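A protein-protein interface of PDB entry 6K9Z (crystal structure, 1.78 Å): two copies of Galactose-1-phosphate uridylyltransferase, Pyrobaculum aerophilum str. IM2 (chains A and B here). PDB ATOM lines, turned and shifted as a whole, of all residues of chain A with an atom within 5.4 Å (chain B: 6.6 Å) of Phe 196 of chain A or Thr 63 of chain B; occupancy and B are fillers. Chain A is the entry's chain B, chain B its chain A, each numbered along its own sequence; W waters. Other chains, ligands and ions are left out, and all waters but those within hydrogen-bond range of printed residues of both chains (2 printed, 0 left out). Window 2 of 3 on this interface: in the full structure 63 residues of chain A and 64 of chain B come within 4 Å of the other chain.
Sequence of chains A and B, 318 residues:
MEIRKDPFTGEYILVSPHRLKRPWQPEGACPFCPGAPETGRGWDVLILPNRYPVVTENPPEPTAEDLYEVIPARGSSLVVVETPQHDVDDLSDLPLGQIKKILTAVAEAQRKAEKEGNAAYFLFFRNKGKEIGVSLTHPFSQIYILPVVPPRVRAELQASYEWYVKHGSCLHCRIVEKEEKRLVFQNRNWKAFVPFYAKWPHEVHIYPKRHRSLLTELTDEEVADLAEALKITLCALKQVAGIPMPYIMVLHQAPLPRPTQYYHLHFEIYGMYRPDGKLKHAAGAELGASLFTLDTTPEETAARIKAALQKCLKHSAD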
ATOM      1  N   GLU A 179       2.231 -16.923  20.232  1.00  0.00           N
ATOM      2  CA  GLU A 179       2.255 -16.555  18.780  1.00  0.00           C
ATOM      3  C   GLU A 179       0.841 -16.602  18.209  1.00  0.00           C
ATOM      4  O   GLU A 179       0.190 -17.655  18.352  1.00  0.00           O
ATOM      5  CB  GLU A 179       3.159 -17.444  17.943  1.00  0.00           C
ATOM      6  CG  GLU A 179       4.603 -17.117  18.155  1.00  0.00           C
ATOM      7  CD  GLU A 179       5.009 -15.785  17.550  1.00  0.00           C
ATOM      8  OE1 GLU A 179       4.470 -15.413  16.482  1.00  0.00           O
ATOM      9  OE2 GLU A 179       5.864 -15.150  18.145  1.00  0.00           O
ATOM     10  N   ARG A 182       1.610 -13.559  14.077  1.00  0.00           N
ATOM     11  CA  ARG A 182       2.590 -14.033  13.060  1.00  0.00           C
ATOM     12  C   ARG A 182       2.428 -15.532  12.805  1.00  0.00           C
ATOM     13  O   ARG A 182       3.276 -16.119  12.107  1.00  0.00           O
ATOM     14  CB  ARG A 182       4.006 -13.683  13.534  1.00  0.00           C
ATOM     15  CG  ARG A 182       4.370 -12.202  13.440  1.00  0.00           C
ATOM     16  CD  ARG A 182       5.842 -11.965  13.777  1.00  0.00           C
ATOM     17  NE  ARG A 182       6.059 -12.456  15.139  1.00  0.00           N
ATOM     18  CZ  ARG A 182       5.774 -11.780  16.241  1.00  0.00           C
ATOM     19  NH1 ARG A 182       5.464 -10.491  16.183  1.00  0.00           N
ATOM     20  NH2 ARG A 182       5.832 -12.390  17.405  1.00  0.00           N
ATOM     21  N   VAL A 194       6.171 -16.902  11.846  1.00  0.00           N
ATOM     22  CA  VAL A 194       7.356 -16.047  11.590  1.00  0.00           C
ATOM     23  C   VAL A 194       7.805 -15.519  12.942  1.00  0.00           C
ATOM     24  O   VAL A 194       7.028 -14.889  13.649  1.00  0.00           O
ATOM     25  CB  VAL A 194       7.008 -14.914  10.619  1.00  0.00           C
ATOM     26  CG1 VAL A 194       8.226 -14.057  10.437  1.00  0.00           C
ATOM     27  CG2 VAL A 194       6.509 -15.396   9.276  1.00  0.00           C
ATOM     28  N   PRO A 195       9.027 -15.834  13.413  1.00  0.00           N
ATOM     29  CA  PRO A 195       9.466 -15.319  14.693  1.00  0.00           C
ATOM     30  C   PRO A 195       9.603 -13.800  14.685  1.00  0.00           C
ATOM     31  O   PRO A 195       9.873 -13.178  13.668  1.00  0.00           O
ATOM     32  CB  PRO A 195      10.822 -15.976  14.929  1.00  0.00           C
ATOM     33  CG  PRO A 195      11.271 -16.430  13.589  1.00  0.00           C
ATOM     34  CD  PRO A 195      10.047 -16.610  12.731  1.00  0.00           C
ATOM     35  N   PHE A 196       9.408 -13.203  15.844  1.00  0.00           N
ATOM     36  CA  PHE A 196       9.593 -11.748  16.013  1.00  0.00           C
ATOM     37  C   PHE A 196      11.009 -11.381  15.556  1.00  0.00           C
ATOM     38  O   PHE A 196      11.203 -10.277  15.050  1.00  0.00           O
ATOM     39  CB  PHE A 196       9.375 -11.386  17.482  1.00  0.00           C
ATOM     40  CG  PHE A 196       9.517  -9.919  17.789  1.00  0.00           C
ATOM     41  CD1 PHE A 196       8.472  -9.035  17.584  1.00  0.00           C
ATOM     42  CD2 PHE A 196      10.722  -9.429  18.253  1.00  0.00           C
ATOM     43  CE1 PHE A 196       8.624  -7.677  17.866  1.00  0.00           C
ATOM     44  CE2 PHE A 196      10.866  -8.082  18.538  1.00  0.00           C
ATOM     45  CZ  PHE A 196       9.811  -7.227  18.366  1.00  0.00           C
ATOM     46  N   TYR A 197      11.953 -12.269  15.865  1.00  0.00           N
ATOM     47  CA  TYR A 197      13.418 -12.130  15.618  1.00  0.00           C
ATOM     48  C   TYR A 197      13.822 -12.802  14.304  1.00  0.00           C
ATOM     49  O   TYR A 197      15.034 -13.195  14.156  1.00  0.00           O
ATOM     50  CB  TYR A 197      14.197 -12.707  16.807  1.00  0.00           C
ATOM     51  CG  TYR A 197      13.659 -14.030  17.290  1.00  0.00           C
ATOM     52  CD1 TYR A 197      12.584 -14.073  18.156  1.00  0.00           C
ATOM     53  CD2 TYR A 197      14.178 -15.229  16.850  1.00  0.00           C
ATOM     54  CE1 TYR A 197      12.046 -15.275  18.611  1.00  0.00           C
ATOM     55  CE2 TYR A 197      13.618 -16.437  17.237  1.00  0.00           C
ATOM     56  CZ  TYR A 197      12.589 -16.465  18.172  1.00  0.00           C
ATOM     57  OH  TYR A 197      12.000 -17.648  18.515  1.00  0.00           O
ATOM     58  N   ALA A 198      12.918 -12.916  13.320  1.00  0.00           N
ATOM     59  CA  ALA A 198      13.292 -13.404  11.965  1.00  0.00           C
ATOM     60  C   ALA A 198      14.486 -12.584  11.436  1.00  0.00           C
ATOM     61  O   ALA A 198      14.482 -11.374  11.566  1.00  0.00           O
ATOM     62  CB  ALA A 198      12.139 -13.288  10.983  1.00  0.00           C
ATOM     63  N   PRO A 298       8.575  -8.606   9.992  1.00  0.00           N
ATOM     64  CA  PRO A 298       8.107  -9.986  10.203  1.00  0.00           C
ATOM     65  C   PRO A 298       6.569 -10.122  10.201  1.00  0.00           C
ATOM     66  O   PRO A 298       5.974 -11.141   9.832  1.00  0.00           O
ATOM     67  CB  PRO A 298       8.703 -10.364  11.560  1.00  0.00           C
ATOM     68  CG  PRO A 298      10.043  -9.595  11.570  1.00  0.00           C
ATOM     69  CD  PRO A 298       9.671  -8.268  10.939  1.00  0.00           C
ATOM     70  N   GLU A 299       5.920  -9.088  10.703  1.00  0.00           N
ATOM     71  CA  GLU A 299       4.448  -9.111  10.802  1.00  0.00           C
ATOM     72  C   GLU A 299       3.874  -9.113   9.342  1.00  0.00           C
ATOM     73  O   GLU A 299       2.836  -9.786   9.101  1.00  0.00           O
ATOM     74  CB  GLU A 299       3.975  -7.954  11.687  1.00  0.00           C
ATOM     75  CG  GLU A 299       4.441  -8.072  13.139  1.00  0.00           C
ATOM     76  CD  GLU A 299       5.932  -7.750  13.366  1.00  0.00           C
ATOM     77  OE1 GLU A 299       6.446  -6.805  12.703  1.00  0.00           O
ATOM     78  OE2 GLU A 299       6.553  -8.477  14.171  1.00  0.00           O
ATOM     79  N   MET B   1      10.563   0.741  12.067  1.00  0.00           N
ATOM     80  CA  MET B   1      12.036   0.637  11.890  1.00  0.00           C
ATOM     81  C   MET B   1      12.703   0.552  13.266  1.00  0.00           C
ATOM     82  O   MET B   1      12.549   1.492  14.056  1.00  0.00           O
ATOM     83  CB  MET B   1      12.588   1.852  11.143  1.00  0.00           C
ATOM     84  CG  MET B   1      14.097   1.838  11.021  1.00  0.00           C
ATOM     85  SD  MET B   1      14.758   3.510  10.927  1.00  0.00           S
ATOM     86  CE  MET B   1      16.364   3.205  10.195  1.00  0.00           C
ATOM     87  N   GLU B   2      13.399  -0.552  13.537  1.00  0.00           N
ATOM     88  CA  GLU B   2      14.051  -0.747  14.858  1.00  0.00           C
ATOM     89  C   GLU B   2      15.091  -1.870  14.788  1.00  0.00           C
ATOM     90  O   GLU B   2      15.195  -2.539  13.747  1.00  0.00           O
ATOM     91  CB  GLU B   2      13.005  -1.123  15.904  1.00  0.00           C
ATOM     92  CG  GLU B   2      12.395  -2.489  15.665  1.00  0.00           C
ATOM     93  CD  GLU B   2      11.054  -2.452  14.958  1.00  0.00           C
ATOM     94  OE1 GLU B   2      10.330  -1.462  15.133  1.00  0.00           O
ATOM     95  OE2 GLU B   2      10.745  -3.411  14.234  1.00  0.00           O
ATOM     96  N   ARG B   4      15.831  -5.371  16.334  1.00  0.00           N
ATOM     97  CA  ARG B   4      15.302  -6.465  17.171  1.00  0.00           C
ATOM     98  C   ARG B   4      16.434  -7.379  17.598  1.00  0.00           C
ATOM     99  O   ARG B   4      17.472  -7.455  16.919  1.00  0.00           O
ATOM    100  CB  ARG B   4      14.171  -7.188  16.422  1.00  0.00           C
ATOM    101  CG  ARG B   4      13.061  -6.286  15.921  1.00  0.00           C
ATOM    102  CD  ARG B   4      11.927  -7.097  15.354  1.00  0.00           C
ATOM    103  NE  ARG B   4      10.878  -6.249  14.894  1.00  0.00           N
ATOM    104  CZ  ARG B   4       9.687  -6.663  14.498  1.00  0.00           C
ATOM    105  NH1 ARG B   4       9.368  -7.951  14.554  1.00  0.00           N
ATOM    106  NH2 ARG B   4       8.799  -5.789  14.073  1.00  0.00           N
ATOM    107  N   LYS B   5      16.253  -8.088  18.714  1.00  0.00           N
ATOM    108  CA  LYS B   5      17.293  -9.001  19.222  1.00  0.00           C
ATOM    109  C   LYS B   5      16.727 -10.414  19.313  1.00  0.00           C
ATOM    110  O   LYS B   5      15.618 -10.605  19.806  1.00  0.00           O
ATOM    111  CB  LYS B   5      17.845  -8.495  20.547  1.00  0.00           C
ATOM    112  CG  LYS B   5      18.969  -9.298  21.113  1.00  0.00           C
ATOM    113  CD  LYS B   5      19.494  -8.590  22.325  1.00  0.00           C
ATOM    114  CE  LYS B   5      20.393  -9.448  23.160  1.00  0.00           C
ATOM    115  NZ  LYS B   5      21.017  -8.618  24.205  1.00  0.00           N
ATOM    116  N   ILE B  13      18.739  -7.795  14.492  1.00  0.00           N
ATOM    117  CA  ILE B  13      18.145  -7.619  13.155  1.00  0.00           C
ATOM    118  C   ILE B  13      17.782  -6.134  13.003  1.00  0.00           C
ATOM    119  O   ILE B  13      16.956  -5.617  13.795  1.00  0.00           O
ATOM    120  CB  ILE B  13      16.932  -8.546  12.944  1.00  0.00           C
ATOM    121  CG1 ILE B  13      17.275  -9.992  13.362  1.00  0.00           C
ATOM    122  CG2 ILE B  13      16.445  -8.487  11.510  1.00  0.00           C
ATOM    123  CD1 ILE B  13      16.987 -10.314  14.817  1.00  0.00           C
ATOM    124  N   VAL B  15      15.526  -3.972  11.294  1.00  0.00           N
ATOM    125  CA  VAL B  15      14.221  -4.073  10.584  1.00  0.00           C
ATOM    126  C   VAL B  15      13.901  -2.673  10.029  1.00  0.00           C
ATOM    127  O   VAL B  15      13.713  -1.787  10.869  1.00  0.00           O
ATOM    128  CB  VAL B  15      13.132  -4.595  11.545  1.00  0.00           C
ATOM    129  CG1 VAL B  15      11.796  -4.701  10.839  1.00  0.00           C
ATOM    130  CG2 VAL B  15      13.518  -5.939  12.132  1.00  0.00           C
ATOM    131  N   PRO B  60      12.595   6.170  14.705  1.00  0.00           N
ATOM    132  CA  PRO B  60      11.319   6.213  15.407  1.00  0.00           C
ATOM    133  C   PRO B  60      11.343   5.349  16.686  1.00  0.00           C
ATOM    134  O   PRO B  60      12.298   4.575  16.937  1.00  0.00           O
ATOM    135  CB  PRO B  60      10.320   5.677  14.379  1.00  0.00           C
ATOM    136  CG  PRO B  60      11.170   4.721  13.582  1.00  0.00           C
ATOM    137  CD  PRO B  60      12.547   5.323  13.501  1.00  0.00           C
ATOM    138  N   GLU B  61      10.248   5.466  17.445  1.00  0.00           N
ATOM    139  CA  GLU B  61       9.995   4.587  18.611  1.00  0.00           C
ATOM    140  C   GLU B  61       9.977   3.140  18.109  1.00  0.00           C
ATOM    141  O   GLU B  61       9.310   2.808  17.127  1.00  0.00           O
ATOM    142  CB  GLU B  61       8.715   5.020  19.331  1.00  0.00           C
ATOM    143  CG  GLU B  61       8.298   4.067  20.438  1.00  0.00           C
ATOM    144  CD  GLU B  61       7.061   4.502  21.213  1.00  0.00           C
ATOM    145  OE1 GLU B  61       6.922   5.725  21.474  1.00  0.00           O
ATOM    146  OE2 GLU B  61       6.227   3.618  21.549  1.00  0.00           O
ATOM    147  N   PRO B  62      10.781   2.238  18.705  1.00  0.00           N
ATOM    148  CA  PRO B  62      10.773   0.842  18.264  1.00  0.00           C
ATOM    149  C   PRO B  62       9.488   0.062  18.591  1.00  0.00           C
ATOM    150  O   PRO B  62       8.818   0.370  19.556  1.00  0.00           O
ATOM    151  CB  PRO B  62      12.024   0.245  18.929  1.00  0.00           C
ATOM    152  CG  PRO B  62      12.384   1.159  20.073  1.00  0.00           C
ATOM    153  CD  PRO B  62      11.786   2.512  19.745  1.00  0.00           C
ATOM    154  N   THR B  63       9.142  -0.886  17.719  1.00  0.00           N
ATOM    155  CA  THR B  63       8.030  -1.864  17.917  1.00  0.00           C
ATOM    156  C   THR B  63       8.340  -2.724  19.145  1.00  0.00           C
ATOM    157  O   THR B  63       9.305  -3.471  19.053  1.00  0.00           O
ATOM    158  CB  THR B  63       7.832  -2.726  16.668  1.00  0.00           C
ATOM    159  OG1 THR B  63       7.895  -1.860  15.527  1.00  0.00           O
ATOM    160  CG2 THR B  63       6.527  -3.497  16.671  1.00  0.00           C
ATOM    161  N   ALA B  64       7.480  -2.685  20.164  1.00  0.00           N
ATOM    162  CA  ALA B  64       7.724  -3.430  21.418  1.00  0.00           C
ATOM    163  C   ALA B  64       6.788  -4.639  21.558  1.00  0.00           C
ATOM    164  O   ALA B  64       5.579  -4.493  21.313  1.00  0.00           O
ATOM    165  CB  ALA B  64       7.573  -2.491  22.587  1.00  0.00           C
ATOM    166  N   GLU B  65       7.368  -5.791  21.910  1.00  0.00           N
ATOM    167  CA  GLU B  65       6.637  -7.056  22.205  1.00  0.00           C
ATOM    168  C   GLU B  65       7.134  -7.532  23.577  1.00  0.00           C
ATOM    169  O   GLU B  65       8.340  -7.404  23.838  1.00  0.00           O
ATOM    170  CB  GLU B  65       6.720  -8.072  21.063  1.00  0.00           C
ATOM    171  CG  GLU B  65       5.387  -8.747  20.792  1.00  0.00           C
ATOM    172  CD  GLU B  65       5.254  -9.505  19.481  1.00  0.00           C
ATOM    173  OE1 GLU B  65       5.128  -8.852  18.433  1.00  0.00           O
ATOM    174  OE2 GLU B  65       5.258 -10.749  19.518  1.00  0.00           O
ATOM    175  N   TYR B  68      10.497  -9.690  24.242  1.00  0.00           N
ATOM    176  CA  TYR B  68      11.584  -9.385  23.273  1.00  0.00           C
ATOM    177  C   TYR B  68      12.214  -8.031  23.551  1.00  0.00           C
ATOM    178  O   TYR B  68      11.474  -7.075  23.979  1.00  0.00           O
ATOM    179  CB  TYR B  68      11.084  -9.405  21.827  1.00  0.00           C
ATOM    180  CG  TYR B  68      10.473 -10.724  21.448  1.00  0.00           C
ATOM    181  CD1 TYR B  68      11.207 -11.897  21.430  1.00  0.00           C
ATOM    182  CD2 TYR B  68       9.113 -10.811  21.206  1.00  0.00           C
ATOM    183  CE1 TYR B  68      10.619 -13.123  21.137  1.00  0.00           C
ATOM    184  CE2 TYR B  68       8.517 -12.017  20.910  1.00  0.00           C
ATOM    185  CZ  TYR B  68       9.267 -13.176  20.856  1.00  0.00           C
ATOM    186  OH  TYR B  68       8.632 -14.345  20.567  1.00  0.00           O
ATOM    187  N   GLU B  69      13.518  -7.934  23.285  1.00  0.00           N
ATOM    188  CA  GLU B  69      14.258  -6.660  23.420  1.00  0.00           C
ATOM    189  C   GLU B  69      14.285  -5.958  22.073  1.00  0.00           C
ATOM    190  O   GLU B  69      14.676  -6.592  21.070  1.00  0.00           O
ATOM    191  CB  GLU B  69      15.681  -6.888  23.910  1.00  0.00           C
ATOM    192  CG  GLU B  69      15.704  -7.427  25.336  1.00  0.00           C
ATOM    193  CD  GLU B  69      17.131  -7.656  25.809  1.00  0.00           C
ATOM    194  OE1 GLU B  69      17.816  -6.651  26.153  1.00  0.00           O
ATOM    195  OE2 GLU B  69      17.590  -8.815  25.722  1.00  0.00           O
ATOM    196  N   VAL B  70      13.919  -4.680  22.056  1.00  0.00           N
ATOM    197  CA  VAL B  70      14.002  -3.870  20.810  1.00  0.00           C
ATOM    198  C   VAL B  70      14.727  -2.571  21.170  1.00  0.00           C
ATOM    199  O   VAL B  70      14.493  -2.053  22.274  1.00  0.00           O
ATOM    200  CB  VAL B  70      12.615  -3.625  20.189  1.00  0.00           C
ATOM    201  CG1 VAL B  70      12.717  -2.848  18.888  1.00  0.00           C
ATOM    202  CG2 VAL B  70      11.886  -4.937  19.962  1.00  0.00           C
ATOM    203  N   ILE B  71      15.609  -2.097  20.296  1.00  0.00           N
ATOM    204  CA  ILE B  71      16.348  -0.838  20.590  1.00  0.00           C
ATOM    205  C   ILE B  71      16.234   0.094  19.383  1.00  0.00           C
ATOM    206  O   ILE B  71      16.070  -0.400  18.252  1.00  0.00           O
ATOM    207  CB  ILE B  71      17.813  -1.119  20.974  1.00  0.00           C
ATOM    208  CG1 ILE B  71      18.602  -1.738  19.821  1.00  0.00           C
ATOM    209  CG2 ILE B  71      17.896  -1.970  22.230  1.00  0.00           C
ATOM    210  CD1 ILE B  71      20.096  -1.663  20.012  1.00  0.00           C
HETATM  211  O   HOH W   1       8.481 -14.911  17.829  1.00  0.00           O
HETATM  212  O   HOH W   2       6.088 -14.685  20.697  1.00  0.00           O
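Water W2 bridges OH of Tyr 68 of chain B (2.6 Å) and OE2 of Glu 179 of chain A (2.6 Å).
Water W1 lies within hydrogen-bond range of the side-chain carboxylate of Glu 179 of chain A (2.6 Å), the backbone NH of Phe 196 of chain A (2.8 Å) and the side-chain hydroxyl of Tyr 68 of chain B (2.8 Å).
Among the printed residues, merely in contact across the chains: Phe 196 of chain A with Glu 65 of chain B (3.5 Å), Phe 196 of chain A with Tyr 68 of chain B (3.5 Å), Pro 298 of chain A with Arg 4 of chain B (3.5 Å), Phe 196 of chain A with Val 70 of chain B (3.5 Å), Ala 198 of chain A with Ile 13 of chain B (3.5 Å), Tyr 197 of chain A with Ile 13 of chain B (3.5 Å), Tyr 197 of chain A with Tyr 68 of chain B (3.6 Å), Glu 179 of chain A with Tyr 68 of chain B (3.8 Å), Phe 196 of chain A with Thr 63 of chain B (3.9 Å) and Tyr 197 of chain A with Lys 5 of chain B (3.9 Å).
OE2 of Glu 2 of chain B lies within salt-bridge range of NE of Arg 4 of chain B (2.9 Å).
The backbone carbonyl oxygen of Arg 4 of chain B is in hydrogen-bond range of the backbone NH of Ile 13 of chain B, at 2.8 Å.
The side-chain carboxylate of Glu 69 of chain B is in salt-bridge range of the side-chain amino group of Lys 5 of chain B (3.8 Å).
The side-chain carboxylate (OE2) of Glu 179 of chain A is in salt-bridge range of the guanidinium group (NH2) of Arg 182 of chain A.
O of Arg 182 of chain A is in hydrogen-bond range of N of Val 194 of chain A, at 3.0 Å.
The guanidinium group (NH1) of Arg 182 of chain A is in salt-bridge range of the side-chain carboxylate (OE2) of Glu 299 of chain A, 3.0 Å away.
Of the 16 printed residues of chain B, 7 touch a printed residue of chain A.
Of the 9 printed residues of chain A, 7 touch a printed residue of chain B.
NH1 of Arg 4 of chain B sits at hydrogen-bond distance from O of Phe 196 of chain A (3.0 Å).
The guanidinium group (NH1) of Arg 4 of chain B is in salt-bridge range of the side-chain carboxylate (OE2) of Glu 299 of chain A.
The side-chain carboxylate (OE2) of Glu 65 of chain B lies within salt-bridge range of the guanidinium group (NH2) of Arg 182 of chain A (2.7 Å).
Pro 195 of chain A touches none of the printed residues of chain B.
Phe 196 of chain A touches just these residues of chain B: Arg 4 (3.0 Å), Thr 63 (3.9 Å), Glu 65 (3.5 Å), Tyr 68 (3.5 Å) and Val 70 (3.5 Å).
Of the printed residues of chain A, Arg 4 of chain B touches Phe 196, Pro 298 and Glu 299.
Of the printed residues of chain A, Lys 5 of chain B touches Tyr 197.
Glu 61 of chain B touches none of the printed residues of chain A.
Of chain A, only Phe 196 comes within 4 Å of Thr 63 of chain B.
Of the printed residues of chain A, Val 70 of chain B touches Phe 196 (3.5 Å).
The nearest residue of chain A that does not touch Thr 63 of chain B is Glu 299 of chain A (5.2 Å).
No position is printed for both chains.
Of the 13 pairs that touch across the chains among the printed residues, none has its exchanged pair printed and touching as well.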
